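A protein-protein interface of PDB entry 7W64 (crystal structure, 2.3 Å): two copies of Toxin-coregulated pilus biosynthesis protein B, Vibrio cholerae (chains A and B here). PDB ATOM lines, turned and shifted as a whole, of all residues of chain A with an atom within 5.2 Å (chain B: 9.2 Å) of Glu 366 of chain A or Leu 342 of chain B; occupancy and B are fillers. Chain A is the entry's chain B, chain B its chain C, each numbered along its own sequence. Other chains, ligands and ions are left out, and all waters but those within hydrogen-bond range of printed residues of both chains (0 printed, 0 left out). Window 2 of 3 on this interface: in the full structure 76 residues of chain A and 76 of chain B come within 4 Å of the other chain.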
ATOM      1  N   HIS A 340      10.807   9.636  30.871  1.00  0.00           N
ATOM      2  CA  HIS A 340      10.026   9.101  29.769  1.00  0.00           C
ATOM      3  C   HIS A 340       9.751  10.210  28.760  1.00  0.00           C
ATOM      4  O   HIS A 340       9.163  11.239  29.108  1.00  0.00           O
ATOM      5  CB  HIS A 340       8.725   8.484  30.291  1.00  0.00           C
ATOM      6  CG  HIS A 340       8.911   7.148  30.961  1.00  0.00           C
ATOM      7  ND1 HIS A 340       9.202   7.013  32.302  1.00  0.00           N
ATOM      8  CD2 HIS A 340       8.857   5.888  30.464  1.00  0.00           C
ATOM      9  CE1 HIS A 340       9.326   5.728  32.599  1.00  0.00           C
ATOM     10  NE2 HIS A 340       9.130   5.025  31.498  1.00  0.00           N
ATOM     11  N   ALA A 341      10.205  10.014  27.523  1.00  0.00           N
ATOM     12  CA  ALA A 341       9.890  10.939  26.449  1.00  0.00           C
ATOM     13  C   ALA A 341       8.409  10.899  26.089  1.00  0.00           C
ATOM     14  O   ALA A 341       7.661   9.954  26.419  1.00  0.00           O
ATOM     15  CB  ALA A 341      10.712  10.633  25.197  1.00  0.00           C
ATOM     16  N   LEU A 342       7.998  11.936  25.374  1.00  0.00           N
ATOM     17  CA  LEU A 342       6.638  12.093  24.894  1.00  0.00           C
ATOM     18  C   LEU A 342       6.406  11.313  23.599  1.00  0.00           C
ATOM     19  O   LEU A 342       7.342  10.981  22.861  1.00  0.00           O
ATOM     20  CB  LEU A 342       6.330  13.571  24.688  1.00  0.00           C
ATOM     21  CG  LEU A 342       6.343  14.284  26.033  1.00  0.00           C
ATOM     22  CD1 LEU A 342       6.159  15.769  25.819  1.00  0.00           C
ATOM     23  CD2 LEU A 342       5.215  13.671  26.940  1.00  0.00           C
ATOM     24  N   LEU A 343       5.129  11.021  23.339  1.00  0.00           N
ATOM     25  CA  LEU A 343       4.704  10.060  22.334  1.00  0.00           C
ATOM     26  C   LEU A 343       3.977  10.733  21.177  1.00  0.00           C
ATOM     27  O   LEU A 343       3.262  11.720  21.365  1.00  0.00           O
ATOM     28  CB  LEU A 343       3.777   8.997  22.970  1.00  0.00           C
ATOM     29  CG  LEU A 343       3.387   7.850  22.038  1.00  0.00           C
ATOM     30  CD1 LEU A 343       3.408   6.534  22.782  1.00  0.00           C
ATOM     31  CD2 LEU A 343       2.061   8.079  21.384  1.00  0.00           C
ATOM     32  N   SER A 344       4.120  10.161  19.984  1.00  0.00           N
ATOM     33  CA  SER A 344       3.374  10.610  18.814  1.00  0.00           C
ATOM     34  C   SER A 344       2.644   9.509  18.067  1.00  0.00           C
ATOM     35  O   SER A 344       1.775   9.823  17.248  1.00  0.00           O
ATOM     36  CB  SER A 344       4.298  11.364  17.823  1.00  0.00           C
ATOM     37  OG  SER A 344       5.276  10.533  17.220  1.00  0.00           O
ATOM     38  N   GLY A 364       6.477   5.761  18.251  1.00  0.00           N
ATOM     39  CA  GLY A 364       7.032   7.019  17.804  1.00  0.00           C
ATOM     40  C   GLY A 364       7.043   7.990  18.964  1.00  0.00           C
ATOM     41  O   GLY A 364       6.055   8.095  19.710  1.00  0.00           O
ATOM     42  N   ILE A 365       8.203   8.641  19.162  1.00  0.00           N
ATOM     43  CA  ILE A 365       8.440   9.554  20.274  1.00  0.00           C
ATOM     44  C   ILE A 365       9.077  10.848  19.769  1.00  0.00           C
ATOM     45  O   ILE A 365       9.494  10.963  18.614  1.00  0.00           O
ATOM     46  CB  ILE A 365       9.312   8.917  21.361  1.00  0.00           C
ATOM     47  CG1 ILE A 365      10.761   8.843  20.912  1.00  0.00           C
ATOM     48  CG2 ILE A 365       8.764   7.482  21.734  1.00  0.00           C
ATOM     49  CD1 ILE A 365      11.674   8.564  22.030  1.00  0.00           C
ATOM     50  N   GLU A 366       9.177  11.819  20.674  1.00  0.00           N
ATOM     51  CA  GLU A 366       9.755  13.100  20.313  1.00  0.00           C
ATOM     52  C   GLU A 366      11.202  12.941  19.853  1.00  0.00           C
ATOM     53  O   GLU A 366      11.973  12.143  20.393  1.00  0.00           O
ATOM     54  CB  GLU A 366       9.650  14.077  21.485  1.00  0.00           C
ATOM     55  CG  GLU A 366      10.020  13.481  22.815  1.00  0.00           C
ATOM     56  CD  GLU A 366      10.045  14.514  23.927  1.00  0.00           C
ATOM     57  OE1 GLU A 366      10.496  15.645  23.658  1.00  0.00           O
ATOM     58  OE2 GLU A 366       9.623  14.195  25.064  1.00  0.00           O
ATOM     59  N   SER A 367      11.564  13.710  18.837  1.00  0.00           N
ATOM     60  CA  SER A 367      12.907  13.650  18.277  1.00  0.00           C
ATOM     61  C   SER A 367      13.908  14.403  19.153  1.00  0.00           C
ATOM     62  O   SER A 367      13.540  15.154  20.058  1.00  0.00           O
ATOM     63  CB  SER A 367      12.897  14.265  16.893  1.00  0.00           C
ATOM     64  OG  SER A 367      12.322  15.549  17.008  1.00  0.00           O
ATOM     65  N   GLY A 368      15.192  14.224  18.842  1.00  0.00           N
ATOM     66  CA  GLY A 368      16.243  14.928  19.557  1.00  0.00           C
ATOM     67  C   GLY A 368      16.560  14.411  20.942  1.00  0.00           C
ATOM     68  O   GLY A 368      17.054  15.180  21.765  1.00  0.00           O
ATOM     69  N   ILE A 369      16.253  13.146  21.243  1.00  0.00           N
ATOM     70  CA  ILE A 369      16.465  12.565  22.574  1.00  0.00           C
ATOM     71  C   ILE A 369      17.231  11.250  22.504  1.00  0.00           C
ATOM     72  O   ILE A 369      18.131  10.993  23.313  1.00  0.00           O
ATOM     73  CB  ILE A 369      15.110  12.396  23.295  1.00  0.00           C
ATOM     74  CG1 ILE A 369      14.616  13.786  23.723  1.00  0.00           C
ATOM     75  CG2 ILE A 369      15.208  11.393  24.478  1.00  0.00           C
ATOM     76  CD1 ILE A 369      13.309  13.842  24.454  1.00  0.00           C
ATOM     77  N   GLY A 378      16.684   7.763  16.568  1.00  0.00           N
ATOM     78  CA  GLY A 378      15.949   8.760  15.815  1.00  0.00           C
ATOM     79  C   GLY A 378      14.717   9.189  16.590  1.00  0.00           C
ATOM     80  O   GLY A 378      14.818   9.852  17.627  1.00  0.00           O
ATOM     81  N   SER A 379      13.538   8.809  16.095  1.00  0.00           N
ATOM     82  CA  SER A 379      12.299   9.027  16.818  1.00  0.00           C
ATOM     83  C   SER A 379      11.525   7.721  17.020  1.00  0.00           C
ATOM     84  O   SER A 379      10.306   7.753  17.242  1.00  0.00           O
ATOM     85  CB  SER A 379      11.440  10.067  16.102  1.00  0.00           C
ATOM     86  OG  SER A 379      12.167  11.248  15.828  1.00  0.00           O
ATOM     87  N   PHE B 310      -2.032   4.022  15.807  1.00  0.00           N
ATOM     88  CA  PHE B 310      -2.348   5.429  15.620  1.00  0.00           C
ATOM     89  C   PHE B 310      -1.054   6.194  15.469  1.00  0.00           C
ATOM     90  O   PHE B 310       0.006   5.756  15.923  1.00  0.00           O
ATOM     91  CB  PHE B 310      -3.125   6.003  16.799  1.00  0.00           C
ATOM     92  CG  PHE B 310      -2.365   5.943  18.079  1.00  0.00           C
ATOM     93  CD1 PHE B 310      -2.421   4.827  18.880  1.00  0.00           C
ATOM     94  CD2 PHE B 310      -1.540   6.977  18.456  1.00  0.00           C
ATOM     95  CE1 PHE B 310      -1.733   4.773  20.055  1.00  0.00           C
ATOM     96  CE2 PHE B 310      -0.824   6.921  19.627  1.00  0.00           C
ATOM     97  CZ  PHE B 310      -0.940   5.819  20.437  1.00  0.00           C
ATOM     98  N   SER B 311      -1.171   7.362  14.832  1.00  0.00           N
ATOM     99  CA  SER B 311      -0.177   8.421  14.873  1.00  0.00           C
ATOM    100  C   SER B 311      -0.897   9.756  14.728  1.00  0.00           C
ATOM    101  O   SER B 311      -2.093   9.815  14.439  1.00  0.00           O
ATOM    102  CB  SER B 311       0.867   8.264  13.766  1.00  0.00           C
ATOM    103  OG  SER B 311       0.338   8.754  12.540  1.00  0.00           O
ATOM    104  N   THR B 312      -0.131  10.840  14.844  1.00  0.00           N
ATOM    105  CA  THR B 312      -0.687  12.183  14.762  1.00  0.00           C
ATOM    106  C   THR B 312      -0.628  12.779  13.356  1.00  0.00           C
ATOM    107  O   THR B 312      -0.652  14.013  13.217  1.00  0.00           O
ATOM    108  CB  THR B 312       0.031  13.096  15.740  1.00  0.00           C
ATOM    109  OG1 THR B 312       1.432  13.108  15.419  1.00  0.00           O
ATOM    110  CG2 THR B 312      -0.181  12.572  17.167  1.00  0.00           C
ATOM    111  N   ALA B 313      -0.519  11.940  12.313  1.00  0.00           N
ATOM    112  CA  ALA B 313      -0.494  12.440  10.939  1.00  0.00           C
ATOM    113  C   ALA B 313      -1.860  12.859  10.426  1.00  0.00           C
ATOM    114  O   ALA B 313      -1.918  13.532   9.392  1.00  0.00           O
ATOM    115  CB  ALA B 313       0.083  11.396   9.975  1.00  0.00           C
ATOM    116  N   THR B 330       2.371  15.538  10.431  1.00  0.00           N
ATOM    117  CA  THR B 330       1.276  16.426  10.779  1.00  0.00           C
ATOM    118  C   THR B 330       1.233  17.660   9.889  1.00  0.00           C
ATOM    119  O   THR B 330       2.252  18.320   9.658  1.00  0.00           O
ATOM    120  CB  THR B 330       1.434  16.870  12.237  1.00  0.00           C
ATOM    121  OG1 THR B 330       1.524  15.723  13.100  1.00  0.00           O
ATOM    122  CG2 THR B 330       0.327  17.848  12.670  1.00  0.00           C
ATOM    123  N   GLN B 332       1.028  21.310   8.913  1.00  0.00           N
ATOM    124  CA  GLN B 332       1.475  22.570   9.502  1.00  0.00           C
ATOM    125  C   GLN B 332       0.516  23.715   9.140  1.00  0.00           C
ATOM    126  O   GLN B 332      -0.466  23.535   8.409  1.00  0.00           O
ATOM    127  CB  GLN B 332       2.893  22.903   9.041  1.00  0.00           C
ATOM    128  CG  GLN B 332       3.867  21.793   9.275  1.00  0.00           C
ATOM    129  CD  GLN B 332       4.046  21.470  10.737  1.00  0.00           C
ATOM    130  OE1 GLN B 332       4.415  22.330  11.541  1.00  0.00           O
ATOM    131  NE2 GLN B 332       3.737  20.222  11.106  1.00  0.00           N
ATOM    132  N   PRO B 339       6.914  17.240  10.806  1.00  0.00           N
ATOM    133  CA  PRO B 339       7.133  16.078  11.669  1.00  0.00           C
ATOM    134  C   PRO B 339       5.843  15.719  12.396  1.00  0.00           C
ATOM    135  O   PRO B 339       4.850  16.448  12.346  1.00  0.00           O
ATOM    136  CB  PRO B 339       8.241  16.530  12.621  1.00  0.00           C
ATOM    137  CG  PRO B 339       8.259  18.035  12.544  1.00  0.00           C
ATOM    138  CD  PRO B 339       7.614  18.458  11.262  1.00  0.00           C
ATOM    139  N   HIS B 340       5.858  14.559  13.062  1.00  0.00           N
ATOM    140  CA  HIS B 340       4.661  14.063  13.769  1.00  0.00           C
ATOM    141  C   HIS B 340       4.484  14.807  15.095  1.00  0.00           C
ATOM    142  O   HIS B 340       5.320  14.691  15.995  1.00  0.00           O
ATOM    143  CB  HIS B 340       4.752  12.544  13.992  1.00  0.00           C
ATOM    144  CG  HIS B 340       4.426  11.724  12.772  1.00  0.00           C
ATOM    145  ND1 HIS B 340       5.365  11.389  11.816  1.00  0.00           N
ATOM    146  CD2 HIS B 340       3.263  11.138  12.377  1.00  0.00           C
ATOM    147  CE1 HIS B 340       4.786  10.677  10.861  1.00  0.00           C
ATOM    148  NE2 HIS B 340       3.510  10.509  11.178  1.00  0.00           N
ATOM    149  N   ALA B 341       3.376  15.526  15.244  1.00  0.00           N
ATOM    150  CA  ALA B 341       3.164  16.239  16.493  1.00  0.00           C
ATOM    151  C   ALA B 341       3.016  15.276  17.658  1.00  0.00           C
ATOM    152  O   ALA B 341       2.741  14.087  17.491  1.00  0.00           O
ATOM    153  CB  ALA B 341       1.910  17.102  16.438  1.00  0.00           C
ATOM    154  N   LEU B 342       3.174  15.825  18.856  1.00  0.00           N
ATOM    155  CA  LEU B 342       3.003  15.057  20.067  1.00  0.00           C
ATOM    156  C   LEU B 342       1.515  14.962  20.429  1.00  0.00           C
ATOM    157  O   LEU B 342       0.694  15.816  20.058  1.00  0.00           O
ATOM    158  CB  LEU B 342       3.821  15.688  21.178  1.00  0.00           C
ATOM    159  CG  LEU B 342       5.305  15.598  20.836  1.00  0.00           C
ATOM    160  CD1 LEU B 342       6.094  16.344  21.874  1.00  0.00           C
ATOM    161  CD2 LEU B 342       5.747  14.124  20.786  1.00  0.00           C
ATOM    162  N   LEU B 343       1.177  13.911  21.174  1.00  0.00           N
ATOM    163  CA  LEU B 343      -0.193  13.472  21.331  1.00  0.00           C
ATOM    164  C   LEU B 343      -0.678  13.727  22.748  1.00  0.00           C
ATOM    165  O   LEU B 343       0.102  13.695  23.703  1.00  0.00           O
ATOM    166  CB  LEU B 343      -0.302  11.984  20.979  1.00  0.00           C
ATOM    167  CG  LEU B 343      -1.683  11.339  21.020  1.00  0.00           C
ATOM    168  CD1 LEU B 343      -1.863  10.465  19.818  1.00  0.00           C
ATOM    169  CD2 LEU B 343      -1.724  10.545  22.257  1.00  0.00           C
ATOM    170  N   SER B 344      -1.968  14.009  22.876  1.00  0.00           N
ATOM    171  CA  SER B 344      -2.560  14.129  24.205  1.00  0.00           C
ATOM    172  C   SER B 344      -3.786  13.247  24.423  1.00  0.00           C
ATOM    173  O   SER B 344      -4.160  13.050  25.581  1.00  0.00           O
ATOM    174  CB  SER B 344      -2.934  15.592  24.525  1.00  0.00           C
ATOM    175  OG  SER B 344      -3.991  16.043  23.698  1.00  0.00           O
ATOM    176  N   GLY B 345      -4.430  12.731  23.384  1.00  0.00           N
ATOM    177  CA  GLY B 345      -5.605  11.890  23.606  1.00  0.00           C
ATOM    178  C   GLY B 345      -6.124  11.309  22.308  1.00  0.00           C
ATOM    179  O   GLY B 345      -5.755  11.743  21.212  1.00  0.00           O
ATOM    180  N   ILE B 363      -8.238  12.608  17.335  1.00  0.00           N
ATOM    181  CA  ILE B 363      -6.910  12.534  17.937  1.00  0.00           C
ATOM    182  C   ILE B 363      -6.540  13.932  18.394  1.00  0.00           C
ATOM    183  O   ILE B 363      -6.446  14.857  17.571  1.00  0.00           O
ATOM    184  CB  ILE B 363      -5.847  11.989  16.971  1.00  0.00           C
ATOM    185  CG1 ILE B 363      -6.129  10.553  16.583  1.00  0.00           C
ATOM    186  CG2 ILE B 363      -4.490  11.984  17.635  1.00  0.00           C
ATOM    187  CD1 ILE B 363      -5.044   9.997  15.696  1.00  0.00           C
ATOM    188  N   GLY B 364      -6.297  14.076  19.695  1.00  0.00           N
ATOM    189  CA  GLY B 364      -5.865  15.339  20.265  1.00  0.00           C
ATOM    190  C   GLY B 364      -4.353  15.444  20.309  1.00  0.00           C
ATOM    191  O   GLY B 364      -3.667  14.530  20.773  1.00  0.00           O
ATOM    192  N   ILE B 365      -3.834  16.561  19.813  1.00  0.00           N
ATOM    193  CA  ILE B 365      -2.403  16.739  19.661  1.00  0.00           C
ATOM    194  C   ILE B 365      -2.002  18.089  20.243  1.00  0.00           C
ATOM    195  O   ILE B 365      -2.846  18.887  20.661  1.00  0.00           O
ATOM    196  CB  ILE B 365      -1.989  16.597  18.185  1.00  0.00           C
ATOM    197  CG1 ILE B 365      -2.430  17.809  17.367  1.00  0.00           C
ATOM    198  CG2 ILE B 365      -2.612  15.322  17.546  1.00  0.00           C
ATOM    199  CD1 ILE B 365      -1.772  17.841  16.002  1.00  0.00           C
ATOM    200  N   GLU B 366      -0.696  18.330  20.296  1.00  0.00           N
ATOM    201  CA  GLU B 366      -0.216  19.623  20.773  1.00  0.00           C
ATOM    202  C   GLU B 366      -0.767  20.735  19.898  1.00  0.00           C
ATOM    203  O   GLU B 366      -0.938  20.573  18.690  1.00  0.00           O
ATOM    204  CB  GLU B 366       1.310  19.681  20.791  1.00  0.00           C
ATOM    205  CG  GLU B 366       1.972  19.187  19.548  1.00  0.00           C
ATOM    206  CD  GLU B 366       3.489  19.348  19.603  1.00  0.00           C
ATOM    207  OE1 GLU B 366       3.980  20.367  20.153  1.00  0.00           O
ATOM    208  OE2 GLU B 366       4.201  18.446  19.108  1.00  0.00           O
ATOM    209  N   SER B 367      -1.103  21.846  20.531  1.00  0.00           N
ATOM    210  CA  SER B 367      -1.650  23.002  19.839  1.00  0.00           C
ATOM    211  C   SER B 367      -0.534  23.817  19.178  1.00  0.00           C
ATOM    212  O   SER B 367       0.663  23.530  19.326  1.00  0.00           O
ATOM    213  CB  SER B 367      -2.420  23.880  20.815  1.00  0.00           C
ATOM    214  OG  SER B 367      -1.565  24.207  21.893  1.00  0.00           O
ATOM    215  N   ILE B 369       0.174  24.142  15.952  1.00  0.00           N
ATOM    216  CA  ILE B 369       0.832  23.528  14.806  1.00  0.00           C
ATOM    217  C   ILE B 369      -0.166  23.447  13.671  1.00  0.00           C
ATOM    218  O   ILE B 369       0.172  23.694  12.514  1.00  0.00           O
ATOM    219  CB  ILE B 369       1.392  22.140  15.157  1.00  0.00           C
ATOM    220  CG1 ILE B 369       2.609  22.263  16.074  1.00  0.00           C
ATOM    221  CG2 ILE B 369       1.744  21.363  13.879  1.00  0.00           C
ATOM    222  CD1 ILE B 369       3.206  20.909  16.457  1.00  0.00           C
ATOM    223  N   LEU B 370      -1.394  23.048  13.975  1.00  0.00           N
ATOM    224  CA  LEU B 370      -2.373  22.861  12.915  1.00  0.00           C
ATOM    225  C   LEU B 370      -2.905  24.207  12.397  1.00  0.00           C
ATOM    226  O   LEU B 370      -2.913  25.199  13.123  1.00  0.00           O
ATOM    227  CB  LEU B 370      -3.515  21.997  13.430  1.00  0.00           C
ATOM    228  CG  LEU B 370      -3.113  20.568  13.803  1.00  0.00           C
ATOM    229  CD1 LEU B 370      -4.232  19.911  14.577  1.00  0.00           C
ATOM    230  CD2 LEU B 370      -2.785  19.796  12.545  1.00  0.00           C
ATOM    231  N   SER B 379      -6.377  21.674  17.820  1.00  0.00           N
ATOM    232  CA  SER B 379      -5.577  20.605  18.407  1.00  0.00           C
ATOM    233  C   SER B 379      -6.171  19.231  18.101  1.00  0.00           C
ATOM    234  O   SER B 379      -5.853  18.252  18.790  1.00  0.00           O
ATOM    235  CB  SER B 379      -5.469  20.773  19.923  1.00  0.00           C
ATOM    236  OG  SER B 379      -5.108  22.076  20.318  1.00  0.00           O
ATOM    237  N   LEU B 380      -7.009  19.127  17.074  1.00  0.00           N
ATOM    238  CA  LEU B 380      -7.756  17.904  16.818  1.00  0.00           C
ATOM    239  C   LEU B 380      -7.519  17.435  15.394  1.00  0.00           C
ATOM    240  O   LEU B 380      -7.537  18.234  14.459  1.00  0.00           O
ATOM    241  CB  LEU B 380      -9.258  18.111  17.015  1.00  0.00           C
ATOM    242  CG  LEU B 380      -9.716  18.410  18.437  1.00  0.00           C
ATOM    243  CD1 LEU B 380     -11.220  18.658  18.431  1.00  0.00           C
ATOM    244  CD2 LEU B 380      -9.347  17.291  19.413  1.00  0.00           C
ATOM    245  N   LEU B 381      -7.321  16.133  15.225  1.00  0.00           N
ATOM    246  CA  LEU B 381      -7.311  15.526  13.905  1.00  0.00           C
ATOM    247  C   LEU B 381      -8.616  14.742  13.839  1.00  0.00           C
ATOM    248  O   LEU B 381      -8.774  13.734  14.546  1.00  0.00           O
ATOM    249  CB  LEU B 381      -6.085  14.633  13.737  1.00  0.00           C
ATOM    250  CG  LEU B 381      -4.773  15.140  14.311  1.00  0.00           C
ATOM    251  CD1 LEU B 381      -3.821  13.973  14.366  1.00  0.00           C
ATOM    252  CD2 LEU B 381      -4.174  16.291  13.458  1.00  0.00           C
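The backbone NH (N) of Leu 343 of chain B is in hydrogen-bond range of the backbone carbonyl oxygen (O) of Leu 343 of chain A (3.0 Å). The backbone carbonyl oxygen (O) of Ser 344 of chain A sits at hydrogen-bond distance from the backbone NH (N) of Thr 312 of chain B, at 3.2 Å.
OE2 of Glu 366 of chain A lies within hydrogen-bond range of N of Leu 342 of chain A (2.8 Å). OG of Ser 311 of chain B sits close to N of Ala 313 of chain B, 3.3 Å away. O of Thr 312 of chain B lies within hydrogen-bond range of OG1 of Thr 330 of chain B. The side-chain hydroxyl (OG1) of Thr 312 of chain B sits at hydrogen-bond distance from the backbone carbonyl oxygen (O) of Ala 341 of chain B, at 2.6 Å. The backbone NH of Ala 341 of chain B sits at hydrogen-bond distance from the side-chain hydroxyl of Thr 330 of chain B (2.8 Å). The side-chain carboxylate (OE2) of Glu 366 of chain B is in hydrogen-bond range of the backbone NH (N) of Leu 342 of chain B, at 2.8 Å.
Leu 342 of chain A touches Leu 342 of chain B. Leu 343 of chain A touches Phe 310 of chain B (CD2 to CE2, 3.6 Å). Leu 342 of chain B touches Leu 343 of chain A. Ser 311 of chain B touches Ser 344 of chain A (CA to O, 3.4 Å). Ser 344 of chain A touches His 340 of chain B. CB of Ser 344 of chain A touches O of Ala 341 of chain B, at 3.2 Å. Glu 366 of chain A touches Leu 342 of chain B.
No residue of chain B comes within 4 Å of Ala 341 of chain A. Of the printed residues of chain B, Ser 344 of chain A touches Ser 311, Thr 312, His 340 and Ala 341. No residue of chain B comes within 4 Å of Ile 365 of chain A. Glu 366 of chain A touches just one residue of chain B: Leu 342. No residue of chain B comes within 4 Å of Ser 367 of chain A. Printed residues of chain A within 4 Å of Thr 312 of chain B: Ser 344 (3.2 Å). Leu 342 of chain B touches three residues of chain A. The nearest residue of chain B that does not touch Glu 366 of chain A is His 340 of chain B (6.4 Å). The nearest printed residue of chain A that does not touch Phe 310 of chain B is Ser 344 of chain A (4.5 Å).
Of the 13 printed residues of chain A, 4 touch a printed residue of chain B. Printed residues of chain A that touch a printed residue of chain B: Leu 342, Leu 343, Ser 344 and Glu 366. Hydrophobic or aromatic side chains of chain A that line the printed part of chain B: Leu 342 and Leu 343. Of the 23 printed residues of chain B, 7 touch a printed residue of chain A. Hydrophobic or aromatic side chains of chain B within 4 Å of the printed part of chain A: Phe 310, His 340, Leu 342 and Leu 343.
Leu 343 of chain A touches Leu 342 of chain B, but with the chains exchanged Leu 342 of chain A does not touch Leu 343 of chain B (6.1 Å). Leu 343 of chain B touches its own counterpart, Leu 343 of chain A. Ser 344 of chain A touches Ala 341 of chain B, but with the chains exchanged Ala 341 of chain A does not touch Ser 344 of chain B (11.0 Å). Glu 366 of chain A touches Leu 342 of chain B, but with the chains exchanged Leu 342 of chain A does not touch Glu 366 of chain B (7.5 Å). Positions printed for both chains: 340, 341, 342, 343, 344, 364, 365, 366, 367, 369 and 379.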
